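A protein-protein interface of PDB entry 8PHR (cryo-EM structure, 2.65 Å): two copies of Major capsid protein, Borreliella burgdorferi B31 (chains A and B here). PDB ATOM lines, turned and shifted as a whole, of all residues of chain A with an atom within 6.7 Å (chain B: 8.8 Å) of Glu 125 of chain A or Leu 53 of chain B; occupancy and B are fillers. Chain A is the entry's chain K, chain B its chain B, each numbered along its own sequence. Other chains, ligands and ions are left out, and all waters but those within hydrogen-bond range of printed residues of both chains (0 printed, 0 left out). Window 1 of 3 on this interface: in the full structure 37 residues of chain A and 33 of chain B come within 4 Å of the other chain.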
ATOM      1  N   TYR A  86     -23.760  21.555 -24.992  1.00  0.00           N
ATOM      2  CA  TYR A  86     -22.779  21.542 -26.067  1.00  0.00           C
ATOM      3  C   TYR A  86     -21.987  20.244 -26.000  1.00  0.00           C
ATOM      4  O   TYR A  86     -21.828  19.653 -24.929  1.00  0.00           O
ATOM      5  CB  TYR A  86     -21.822  22.740 -25.978  1.00  0.00           C
ATOM      6  CG  TYR A  86     -22.205  23.914 -26.853  1.00  0.00           C
ATOM      7  CD1 TYR A  86     -22.300  23.775 -28.231  1.00  0.00           C
ATOM      8  CD2 TYR A  86     -22.464  25.160 -26.300  1.00  0.00           C
ATOM      9  CE1 TYR A  86     -22.644  24.845 -29.034  1.00  0.00           C
ATOM     10  CE2 TYR A  86     -22.811  26.236 -27.096  1.00  0.00           C
ATOM     11  CZ  TYR A  86     -22.900  26.073 -28.462  1.00  0.00           C
ATOM     12  OH  TYR A  86     -23.244  27.139 -29.259  1.00  0.00           O
ATOM     13  N   LYS A 120     -11.432  23.040 -20.728  1.00  0.00           N
ATOM     14  CA  LYS A 120     -11.133  24.422 -20.358  1.00  0.00           C
ATOM     15  C   LYS A 120     -11.522  25.386 -21.473  1.00  0.00           C
ATOM     16  O   LYS A 120     -12.190  26.400 -21.232  1.00  0.00           O
ATOM     17  CB  LYS A 120      -9.651  24.577 -20.017  1.00  0.00           C
ATOM     18  CG  LYS A 120      -9.266  26.010 -19.668  1.00  0.00           C
ATOM     19  CD  LYS A 120      -7.768  26.250 -19.768  1.00  0.00           C
ATOM     20  CE  LYS A 120      -6.991  25.351 -18.824  1.00  0.00           C
ATOM     21  NZ  LYS A 120      -5.523  25.564 -18.942  1.00  0.00           N
ATOM     22  N   LEU A 121     -11.117  25.079 -22.708  1.00  0.00           N
ATOM     23  CA  LEU A 121     -11.431  25.968 -23.824  1.00  0.00           C
ATOM     24  C   LEU A 121     -12.934  26.036 -24.079  1.00  0.00           C
ATOM     25  O   LEU A 121     -13.485  27.122 -24.323  1.00  0.00           O
ATOM     26  CB  LEU A 121     -10.686  25.515 -25.080  1.00  0.00           C
ATOM     27  CG  LEU A 121      -9.161  25.439 -24.979  1.00  0.00           C
ATOM     28  CD1 LEU A 121      -8.547  25.148 -26.340  1.00  0.00           C
ATOM     29  CD2 LEU A 121      -8.592  26.724 -24.397  1.00  0.00           C
ATOM     30  N   ALA A 122     -13.619  24.890 -24.024  1.00  0.00           N
ATOM     31  CA  ALA A 122     -15.063  24.880 -24.234  1.00  0.00           C
ATOM     32  C   ALA A 122     -15.784  25.670 -23.150  1.00  0.00           C
ATOM     33  O   ALA A 122     -16.725  26.416 -23.441  1.00  0.00           O
ATOM     34  CB  ALA A 122     -15.574  23.441 -24.285  1.00  0.00           C
ATOM     35  N   SER A 123     -15.355  25.520 -21.894  1.00  0.00           N
ATOM     36  CA  SER A 123     -15.960  26.277 -20.806  1.00  0.00           C
ATOM     37  C   SER A 123     -15.729  27.770 -20.982  1.00  0.00           C
ATOM     38  O   SER A 123     -16.626  28.576 -20.718  1.00  0.00           O
ATOM     39  CB  SER A 123     -15.405  25.802 -19.463  1.00  0.00           C
ATOM     40  OG  SER A 123     -15.683  24.429 -19.254  1.00  0.00           O
ATOM     41  N   SER A 124     -14.529  28.159 -21.420  1.00  0.00           N
ATOM     42  CA  SER A 124     -14.267  29.573 -21.672  1.00  0.00           C
ATOM     43  C   SER A 124     -15.193  30.119 -22.754  1.00  0.00           C
ATOM     44  O   SER A 124     -15.766  31.207 -22.602  1.00  0.00           O
ATOM     45  CB  SER A 124     -12.804  29.776 -22.064  1.00  0.00           C
ATOM     46  OG  SER A 124     -11.935  29.339 -21.033  1.00  0.00           O
ATOM     47  N   GLU A 125     -15.363  29.370 -23.846  1.00  0.00           N
ATOM     48  CA  GLU A 125     -16.255  29.819 -24.913  1.00  0.00           C
ATOM     49  C   GLU A 125     -17.699  29.916 -24.426  1.00  0.00           C
ATOM     50  O   GLU A 125     -18.416  30.871 -24.758  1.00  0.00           O
ATOM     51  CB  GLU A 125     -16.154  28.879 -26.113  1.00  0.00           C
ATOM     52  CG  GLU A 125     -14.976  29.173 -27.026  1.00  0.00           C
ATOM     53  CD  GLU A 125     -15.196  30.404 -27.883  1.00  0.00           C
ATOM     54  OE1 GLU A 125     -16.173  30.421 -28.661  1.00  0.00           O
ATOM     55  OE2 GLU A 125     -14.393  31.354 -27.778  1.00  0.00           O
ATOM     56  N   ILE A 126     -18.143  28.939 -23.632  1.00  0.00           N
ATOM     57  CA  ILE A 126     -19.515  28.957 -23.135  1.00  0.00           C
ATOM     58  C   ILE A 126     -19.724  30.124 -22.177  1.00  0.00           C
ATOM     59  O   ILE A 126     -20.789  30.748 -22.167  1.00  0.00           O
ATOM     60  CB  ILE A 126     -19.872  27.608 -22.485  1.00  0.00           C
ATOM     61  CG1 ILE A 126     -19.826  26.490 -23.528  1.00  0.00           C
ATOM     62  CG2 ILE A 126     -21.254  27.664 -21.853  1.00  0.00           C
ATOM     63  CD1 ILE A 126     -20.210  25.131 -22.987  1.00  0.00           C
ATOM     64  N   ILE A 127     -18.718  30.445 -21.360  1.00  0.00           N
ATOM     65  CA  ILE A 127     -18.836  31.592 -20.464  1.00  0.00           C
ATOM     66  C   ILE A 127     -18.880  32.891 -21.258  1.00  0.00           C
ATOM     67  O   ILE A 127     -19.610  33.825 -20.902  1.00  0.00           O
ATOM     68  CB  ILE A 127     -17.698  31.588 -19.427  1.00  0.00           C
ATOM     69  CG1 ILE A 127     -17.838  30.385 -18.493  1.00  0.00           C
ATOM     70  CG2 ILE A 127     -17.689  32.881 -18.625  1.00  0.00           C
ATOM     71  CD1 ILE A 127     -16.657  30.183 -17.581  1.00  0.00           C
ATOM     72  N   LYS A 128     -18.107  32.977 -22.343  1.00  0.00           N
ATOM     73  CA  LYS A 128     -18.216  34.137 -23.226  1.00  0.00           C
ATOM     74  C   LYS A 128     -19.632  34.270 -23.775  1.00  0.00           C
ATOM     75  O   LYS A 128     -20.209  35.366 -23.797  1.00  0.00           O
ATOM     76  CB  LYS A 128     -17.206  34.031 -24.370  1.00  0.00           C
ATOM     77  CG  LYS A 128     -15.751  34.077 -23.941  1.00  0.00           C
ATOM     78  CD  LYS A 128     -14.829  34.049 -25.150  1.00  0.00           C
ATOM     79  CE  LYS A 128     -13.369  33.999 -24.733  1.00  0.00           C
ATOM     80  NZ  LYS A 128     -12.460  33.952 -25.911  1.00  0.00           N
ATOM     81  N   LEU A 129     -20.212  33.150 -24.216  1.00  0.00           N
ATOM     82  CA  LEU A 129     -21.577  33.176 -24.738  1.00  0.00           C
ATOM     83  C   LEU A 129     -22.577  33.592 -23.664  1.00  0.00           C
ATOM     84  O   LEU A 129     -23.513  34.355 -23.936  1.00  0.00           O
ATOM     85  CB  LEU A 129     -21.943  31.806 -25.312  1.00  0.00           C
ATOM     86  CG  LEU A 129     -23.374  31.638 -25.831  1.00  0.00           C
ATOM     87  CD1 LEU A 129     -23.503  32.176 -27.249  1.00  0.00           C
ATOM     88  CD2 LEU A 129     -23.804  30.181 -25.764  1.00  0.00           C
ATOM     89  N   ILE A 130     -22.401  33.093 -22.438  1.00  0.00           N
ATOM     90  CA  ILE A 130     -23.304  33.444 -21.344  1.00  0.00           C
ATOM     91  C   ILE A 130     -23.209  34.931 -21.025  1.00  0.00           C
ATOM     92  O   ILE A 130     -24.225  35.593 -20.783  1.00  0.00           O
ATOM     93  CB  ILE A 130     -23.011  32.578 -20.105  1.00  0.00           C
ATOM     94  CG1 ILE A 130     -23.310  31.107 -20.397  1.00  0.00           C
ATOM     95  CG2 ILE A 130     -23.821  33.056 -18.908  1.00  0.00           C
ATOM     96  CD1 ILE A 130     -23.049  30.185 -19.227  1.00  0.00           C
ATOM     97  N   SER A 140     -26.537  34.333 -30.148  1.00  0.00           N
ATOM     98  CA  SER A 140     -26.152  34.160 -31.543  1.00  0.00           C
ATOM     99  C   SER A 140     -24.646  33.961 -31.617  1.00  0.00           C
ATOM    100  O   SER A 140     -23.910  34.297 -30.685  1.00  0.00           O
ATOM    101  CB  SER A 140     -26.582  35.357 -32.398  1.00  0.00           C
ATOM    102  OG  SER A 140     -26.173  35.193 -33.744  1.00  0.00           O
ATOM    103  N   ILE A 141     -24.198  33.405 -32.743  1.00  0.00           N
ATOM    104  CA  ILE A 141     -22.784  33.172 -33.000  1.00  0.00           C
ATOM    105  C   ILE A 141     -22.310  33.873 -34.267  1.00  0.00           C
ATOM    106  O   ILE A 141     -21.230  33.569 -34.772  1.00  0.00           O
ATOM    107  CB  ILE A 141     -22.468  31.664 -33.063  1.00  0.00           C
ATOM    108  CG1 ILE A 141     -23.264  30.999 -34.188  1.00  0.00           C
ATOM    109  CG2 ILE A 141     -22.759  31.003 -31.728  1.00  0.00           C
ATOM    110  CD1 ILE A 141     -22.580  29.788 -34.781  1.00  0.00           C
ATOM    111  N   ASP B  50      -7.208  27.229 -29.489  1.00  0.00           N
ATOM    112  CA  ASP B  50      -8.387  28.062 -29.297  1.00  0.00           C
ATOM    113  C   ASP B  50      -9.632  27.312 -29.748  1.00  0.00           C
ATOM    114  O   ASP B  50      -9.624  26.646 -30.786  1.00  0.00           O
ATOM    115  CB  ASP B  50      -8.264  29.384 -30.065  1.00  0.00           C
ATOM    116  CG  ASP B  50      -9.236  30.437 -29.572  1.00  0.00           C
ATOM    117  OD1 ASP B  50      -9.943  30.176 -28.575  1.00  0.00           O
ATOM    118  OD2 ASP B  50      -9.295  31.525 -30.182  1.00  0.00           O
ATOM    119  N   ALA B  51     -10.703  27.435 -28.969  1.00  0.00           N
ATOM    120  CA  ALA B  51     -11.964  26.770 -29.255  1.00  0.00           C
ATOM    121  C   ALA B  51     -12.961  27.730 -29.891  1.00  0.00           C
ATOM    122  O   ALA B  51     -12.825  28.954 -29.816  1.00  0.00           O
ATOM    123  CB  ALA B  51     -12.566  26.172 -27.982  1.00  0.00           C
ATOM    124  N   PHE B  52     -13.983  27.149 -30.519  1.00  0.00           N
ATOM    125  CA  PHE B  52     -15.047  27.918 -31.147  1.00  0.00           C
ATOM    126  C   PHE B  52     -16.315  27.077 -31.175  1.00  0.00           C
ATOM    127  O   PHE B  52     -16.272  25.851 -31.067  1.00  0.00           O
ATOM    128  CB  PHE B  52     -14.655  28.367 -32.562  1.00  0.00           C
ATOM    129  CG  PHE B  52     -14.274  27.237 -33.479  1.00  0.00           C
ATOM    130  CD1 PHE B  52     -15.237  26.552 -34.202  1.00  0.00           C
ATOM    131  CD2 PHE B  52     -12.947  26.862 -33.619  1.00  0.00           C
ATOM    132  CE1 PHE B  52     -14.885  25.515 -35.046  1.00  0.00           C
ATOM    133  CE2 PHE B  52     -12.590  25.826 -34.462  1.00  0.00           C
ATOM    134  CZ  PHE B  52     -13.559  25.151 -35.175  1.00  0.00           C
ATOM    135  N   LEU B  53     -17.450  27.753 -31.319  1.00  0.00           N
ATOM    136  CA  LEU B  53     -18.753  27.105 -31.392  1.00  0.00           C
ATOM    137  C   LEU B  53     -19.163  26.975 -32.853  1.00  0.00           C
ATOM    138  O   LEU B  53     -19.043  27.938 -33.618  1.00  0.00           O
ATOM    139  CB  LEU B  53     -19.802  27.908 -30.620  1.00  0.00           C
ATOM    140  CG  LEU B  53     -19.424  28.372 -29.211  1.00  0.00           C
ATOM    141  CD1 LEU B  53     -20.521  29.250 -28.625  1.00  0.00           C
ATOM    142  CD2 LEU B  53     -19.143  27.188 -28.305  1.00  0.00           C
ATOM    143  N   ASN B  54     -19.649  25.793 -33.242  1.00  0.00           N
ATOM    144  CA  ASN B  54     -20.035  25.582 -34.630  1.00  0.00           C
ATOM    145  C   ASN B  54     -21.502  25.889 -34.897  1.00  0.00           C
ATOM    146  O   ASN B  54     -21.878  26.079 -36.059  1.00  0.00           O
ATOM    147  CB  ASN B  54     -19.734  24.139 -35.047  1.00  0.00           C
ATOM    148  CG  ASN B  54     -19.513  23.995 -36.539  1.00  0.00           C
ATOM    149  OD1 ASN B  54     -19.617  24.964 -37.291  1.00  0.00           O
ATOM    150  ND2 ASN B  54     -19.206  22.780 -36.976  1.00  0.00           N
ATOM    151  N   ALA B  55     -22.333  25.951 -33.860  1.00  0.00           N
ATOM    152  CA  ALA B  55     -23.752  26.228 -34.028  1.00  0.00           C
ATOM    153  C   ALA B  55     -24.329  26.663 -32.690  1.00  0.00           C
ATOM    154  O   ALA B  55     -23.660  26.617 -31.656  1.00  0.00           O
ATOM    155  CB  ALA B  55     -24.501  25.010 -34.577  1.00  0.00           C
ATOM    156  N   ASN B  56     -25.588  27.092 -32.728  1.00  0.00           N
ATOM    157  CA  ASN B  56     -26.280  27.482 -31.513  1.00  0.00           C
ATOM    158  C   ASN B  56     -26.507  26.265 -30.618  1.00  0.00           C
ATOM    159  O   ASN B  56     -26.660  25.144 -31.109  1.00  0.00           O
ATOM    160  CB  ASN B  56     -27.617  28.138 -31.849  1.00  0.00           C
ATOM    161  CG  ASN B  56     -27.455  29.417 -32.644  1.00  0.00           C
ATOM    162  OD1 ASN B  56     -26.739  30.329 -32.232  1.00  0.00           O
ATOM    163  ND2 ASN B  56     -28.120  29.490 -33.789  1.00  0.00           N
ATOM    164  N   PRO B  57     -26.532  26.458 -29.302  1.00  0.00           N
ATOM    165  CA  PRO B  57     -26.740  25.327 -28.393  1.00  0.00           C
ATOM    166  C   PRO B  57     -28.132  24.732 -28.547  1.00  0.00           C
ATOM    167  O   PRO B  57     -29.059  25.358 -29.065  1.00  0.00           O
ATOM    168  CB  PRO B  57     -26.547  25.941 -27.003  1.00  0.00           C
ATOM    169  CG  PRO B  57     -26.808  27.397 -27.191  1.00  0.00           C
ATOM    170  CD  PRO B  57     -26.344  27.727 -28.576  1.00  0.00           C
ATOM    171  N   SER B  68     -25.166  20.316 -30.677  1.00  0.00           N
ATOM    172  CA  SER B  68     -24.239  21.213 -31.347  1.00  0.00           C
ATOM    173  C   SER B  68     -22.803  20.894 -30.942  1.00  0.00           C
ATOM    174  O   SER B  68     -22.543  20.241 -29.927  1.00  0.00           O
ATOM    175  CB  SER B  68     -24.572  22.668 -31.020  1.00  0.00           C
ATOM    176  OG  SER B  68     -25.826  23.039 -31.564  1.00  0.00           O
ATOM    177  N   THR B  69     -21.860  21.368 -31.752  1.00  0.00           N
ATOM    178  CA  THR B  69     -20.465  20.980 -31.627  1.00  0.00           C
ATOM    179  C   THR B  69     -19.577  22.174 -31.295  1.00  0.00           C
ATOM    180  O   THR B  69     -19.868  23.322 -31.656  1.00  0.00           O
ATOM    181  CB  THR B  69     -19.960  20.309 -32.913  1.00  0.00           C
ATOM    182  OG1 THR B  69     -20.269  21.138 -34.039  1.00  0.00           O
ATOM    183  CG2 THR B  69     -20.615  18.948 -33.094  1.00  0.00           C
ATOM    184  N   ILE B  70     -18.486  21.879 -30.592  1.00  0.00           N
ATOM    185  CA  ILE B  70     -17.447  22.849 -30.273  1.00  0.00           C
ATOM    186  C   ILE B  70     -16.164  22.379 -30.941  1.00  0.00           C
ATOM    187  O   ILE B  70     -15.629  21.320 -30.595  1.00  0.00           O
ATOM    188  CB  ILE B  70     -17.253  23.006 -28.756  1.00  0.00           C
ATOM    189  CG1 ILE B  70     -18.502  23.618 -28.120  1.00  0.00           C
ATOM    190  CG2 ILE B  70     -16.024  23.855 -28.459  1.00  0.00           C
ATOM    191  CD1 ILE B  70     -18.388  23.821 -26.627  1.00  0.00           C
ATOM    192  N   GLY B  71     -15.674  23.163 -31.899  1.00  0.00           N
ATOM    193  CA  GLY B  71     -14.460  22.840 -32.614  1.00  0.00           C
ATOM    194  C   GLY B  71     -13.236  23.509 -32.007  1.00  0.00           C
ATOM    195  O   GLY B  71     -13.329  24.395 -31.163  1.00  0.00           O
ATOM    196  N   PHE B  72     -12.071  23.073 -32.478  1.00  0.00           N
ATOM    197  CA  PHE B  72     -10.794  23.532 -31.958  1.00  0.00           C
ATOM    198  C   PHE B  72      -9.855  23.856 -33.112  1.00  0.00           C
ATOM    199  O   PHE B  72      -9.996  23.336 -34.222  1.00  0.00           O
ATOM    200  CB  PHE B  72     -10.155  22.478 -31.045  1.00  0.00           C
ATOM    201  CG  PHE B  72     -10.974  22.151 -29.829  1.00  0.00           C
ATOM    202  CD1 PHE B  72     -11.020  23.020 -28.753  1.00  0.00           C
ATOM    203  CD2 PHE B  72     -11.700  20.973 -29.766  1.00  0.00           C
ATOM    204  CE1 PHE B  72     -11.775  22.718 -27.633  1.00  0.00           C
ATOM    205  CE2 PHE B  72     -12.457  20.666 -28.650  1.00  0.00           C
ATOM    206  CZ  PHE B  72     -12.494  21.541 -27.583  1.00  0.00           C
ATOM    207  N   ASP B 195     -10.355  40.992 -26.052  1.00  0.00           N
ATOM    208  CA  ASP B 195     -10.918  40.983 -24.709  1.00  0.00           C
ATOM    209  C   ASP B 195      -9.876  41.217 -23.621  1.00  0.00           C
ATOM    210  O   ASP B 195     -10.249  41.387 -22.456  1.00  0.00           O
ATOM    211  CB  ASP B 195     -11.644  39.657 -24.449  1.00  0.00           C
ATOM    212  CG  ASP B 195     -10.719  38.454 -24.526  1.00  0.00           C
ATOM    213  OD1 ASP B 195      -9.536  38.622 -24.888  1.00  0.00           O
ATOM    214  OD2 ASP B 195     -11.180  37.333 -24.224  1.00  0.00           O
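The side-chain hydroxyl of Tyr 86 of chain A sits at hydrogen-bond distance from the backbone carbonyl oxygen of Ala 55 of chain B, 2.5 Å away.
OH of Tyr 86 of chain A sits close to N of Pro 57 of chain B.
The side-chain amino group of Lys 128 of chain A is in salt-bridge range of the side-chain carboxylate of Asp 195 of chain B, at 3.99 Å.
The backbone NH (N) of Asn 54 of chain B sits at hydrogen-bond distance from the backbone carbonyl oxygen (O) of Thr 69 of chain B (2.9 Å).
The backbone carbonyl oxygen of Phe 52 of chain B is in hydrogen-bond range of the backbone NH of Gly 71 of chain B.
The side-chain carboxylate (OE2) of Glu 125 of chain A lies within salt-bridge range of the side-chain amino group (NZ) of Lys 128 of chain A (3.7 Å).
Among the printed residues, merely in contact across the chains: Glu 125 of chain A with Ala 51 of chain B, Tyr 86 of chain A with Leu 53 of chain B, Leu 121 of chain A with Ala 51 of chain B, Tyr 86 of chain A with Ser 68 of chain B, Tyr 86 of chain A with Asn 56 of chain B, Tyr 86 of chain A with Ile 70 of chain B, Ala 122 of chain A with Ile 70 of chain B, Glu 125 of chain A with Phe 52 of chain B, Ile 141 of chain A with Ala 55 of chain B, Glu 125 of chain A with Leu 53 of chain B, Ser 140 of chain A with Asn 56 of chain B, Leu 121 of chain A with Phe 72 of chain B and Ile 141 of chain A with Asn 54 of chain B.
Glu 125 of chain A touches three residues of chain B.
Of the printed residues of chain A, Asn 56 of chain B touches Tyr 86 (3.6 Å) and Ser 140 (3.9 Å).
Printed residues of chain A within 4 Å of Ala 55 of chain B: Tyr 86 (2.5 Å) and Ile 141 (3.8 Å).
Printed residues of chain B within 4 Å of Ile 141 of chain A: Asn 54 and Ala 55.
Of the printed residues of chain A, Ile 70 of chain B touches Tyr 86 (3.7 Å) and Ala 122 (3.7 Å).
The nearest residue of chain B that does not touch Glu 125 of chain A is Asp 50 of chain B (4.7 Å).
Printed residues of chain B that touch a printed residue of chain A: Ala 51, Phe 52, Leu 53, Asn 54, Ala 55, Asn 56, Pro 57, Ser 68, Ile 70, Phe 72 and Asp 195.
Along chain B the printed residues that touch a printed residue of chain A span positions 51 to 195.
Among the printed residues, 16 pairs touch across the chains.
Among the printed residues, Asp or Glu carboxylates within 4 Å of a Lys or Arg side-chain nitrogen of the other chain: Lys 128 of chain A with Asp 195 of chain B (3.99 Å).
No position is printed for both chains.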
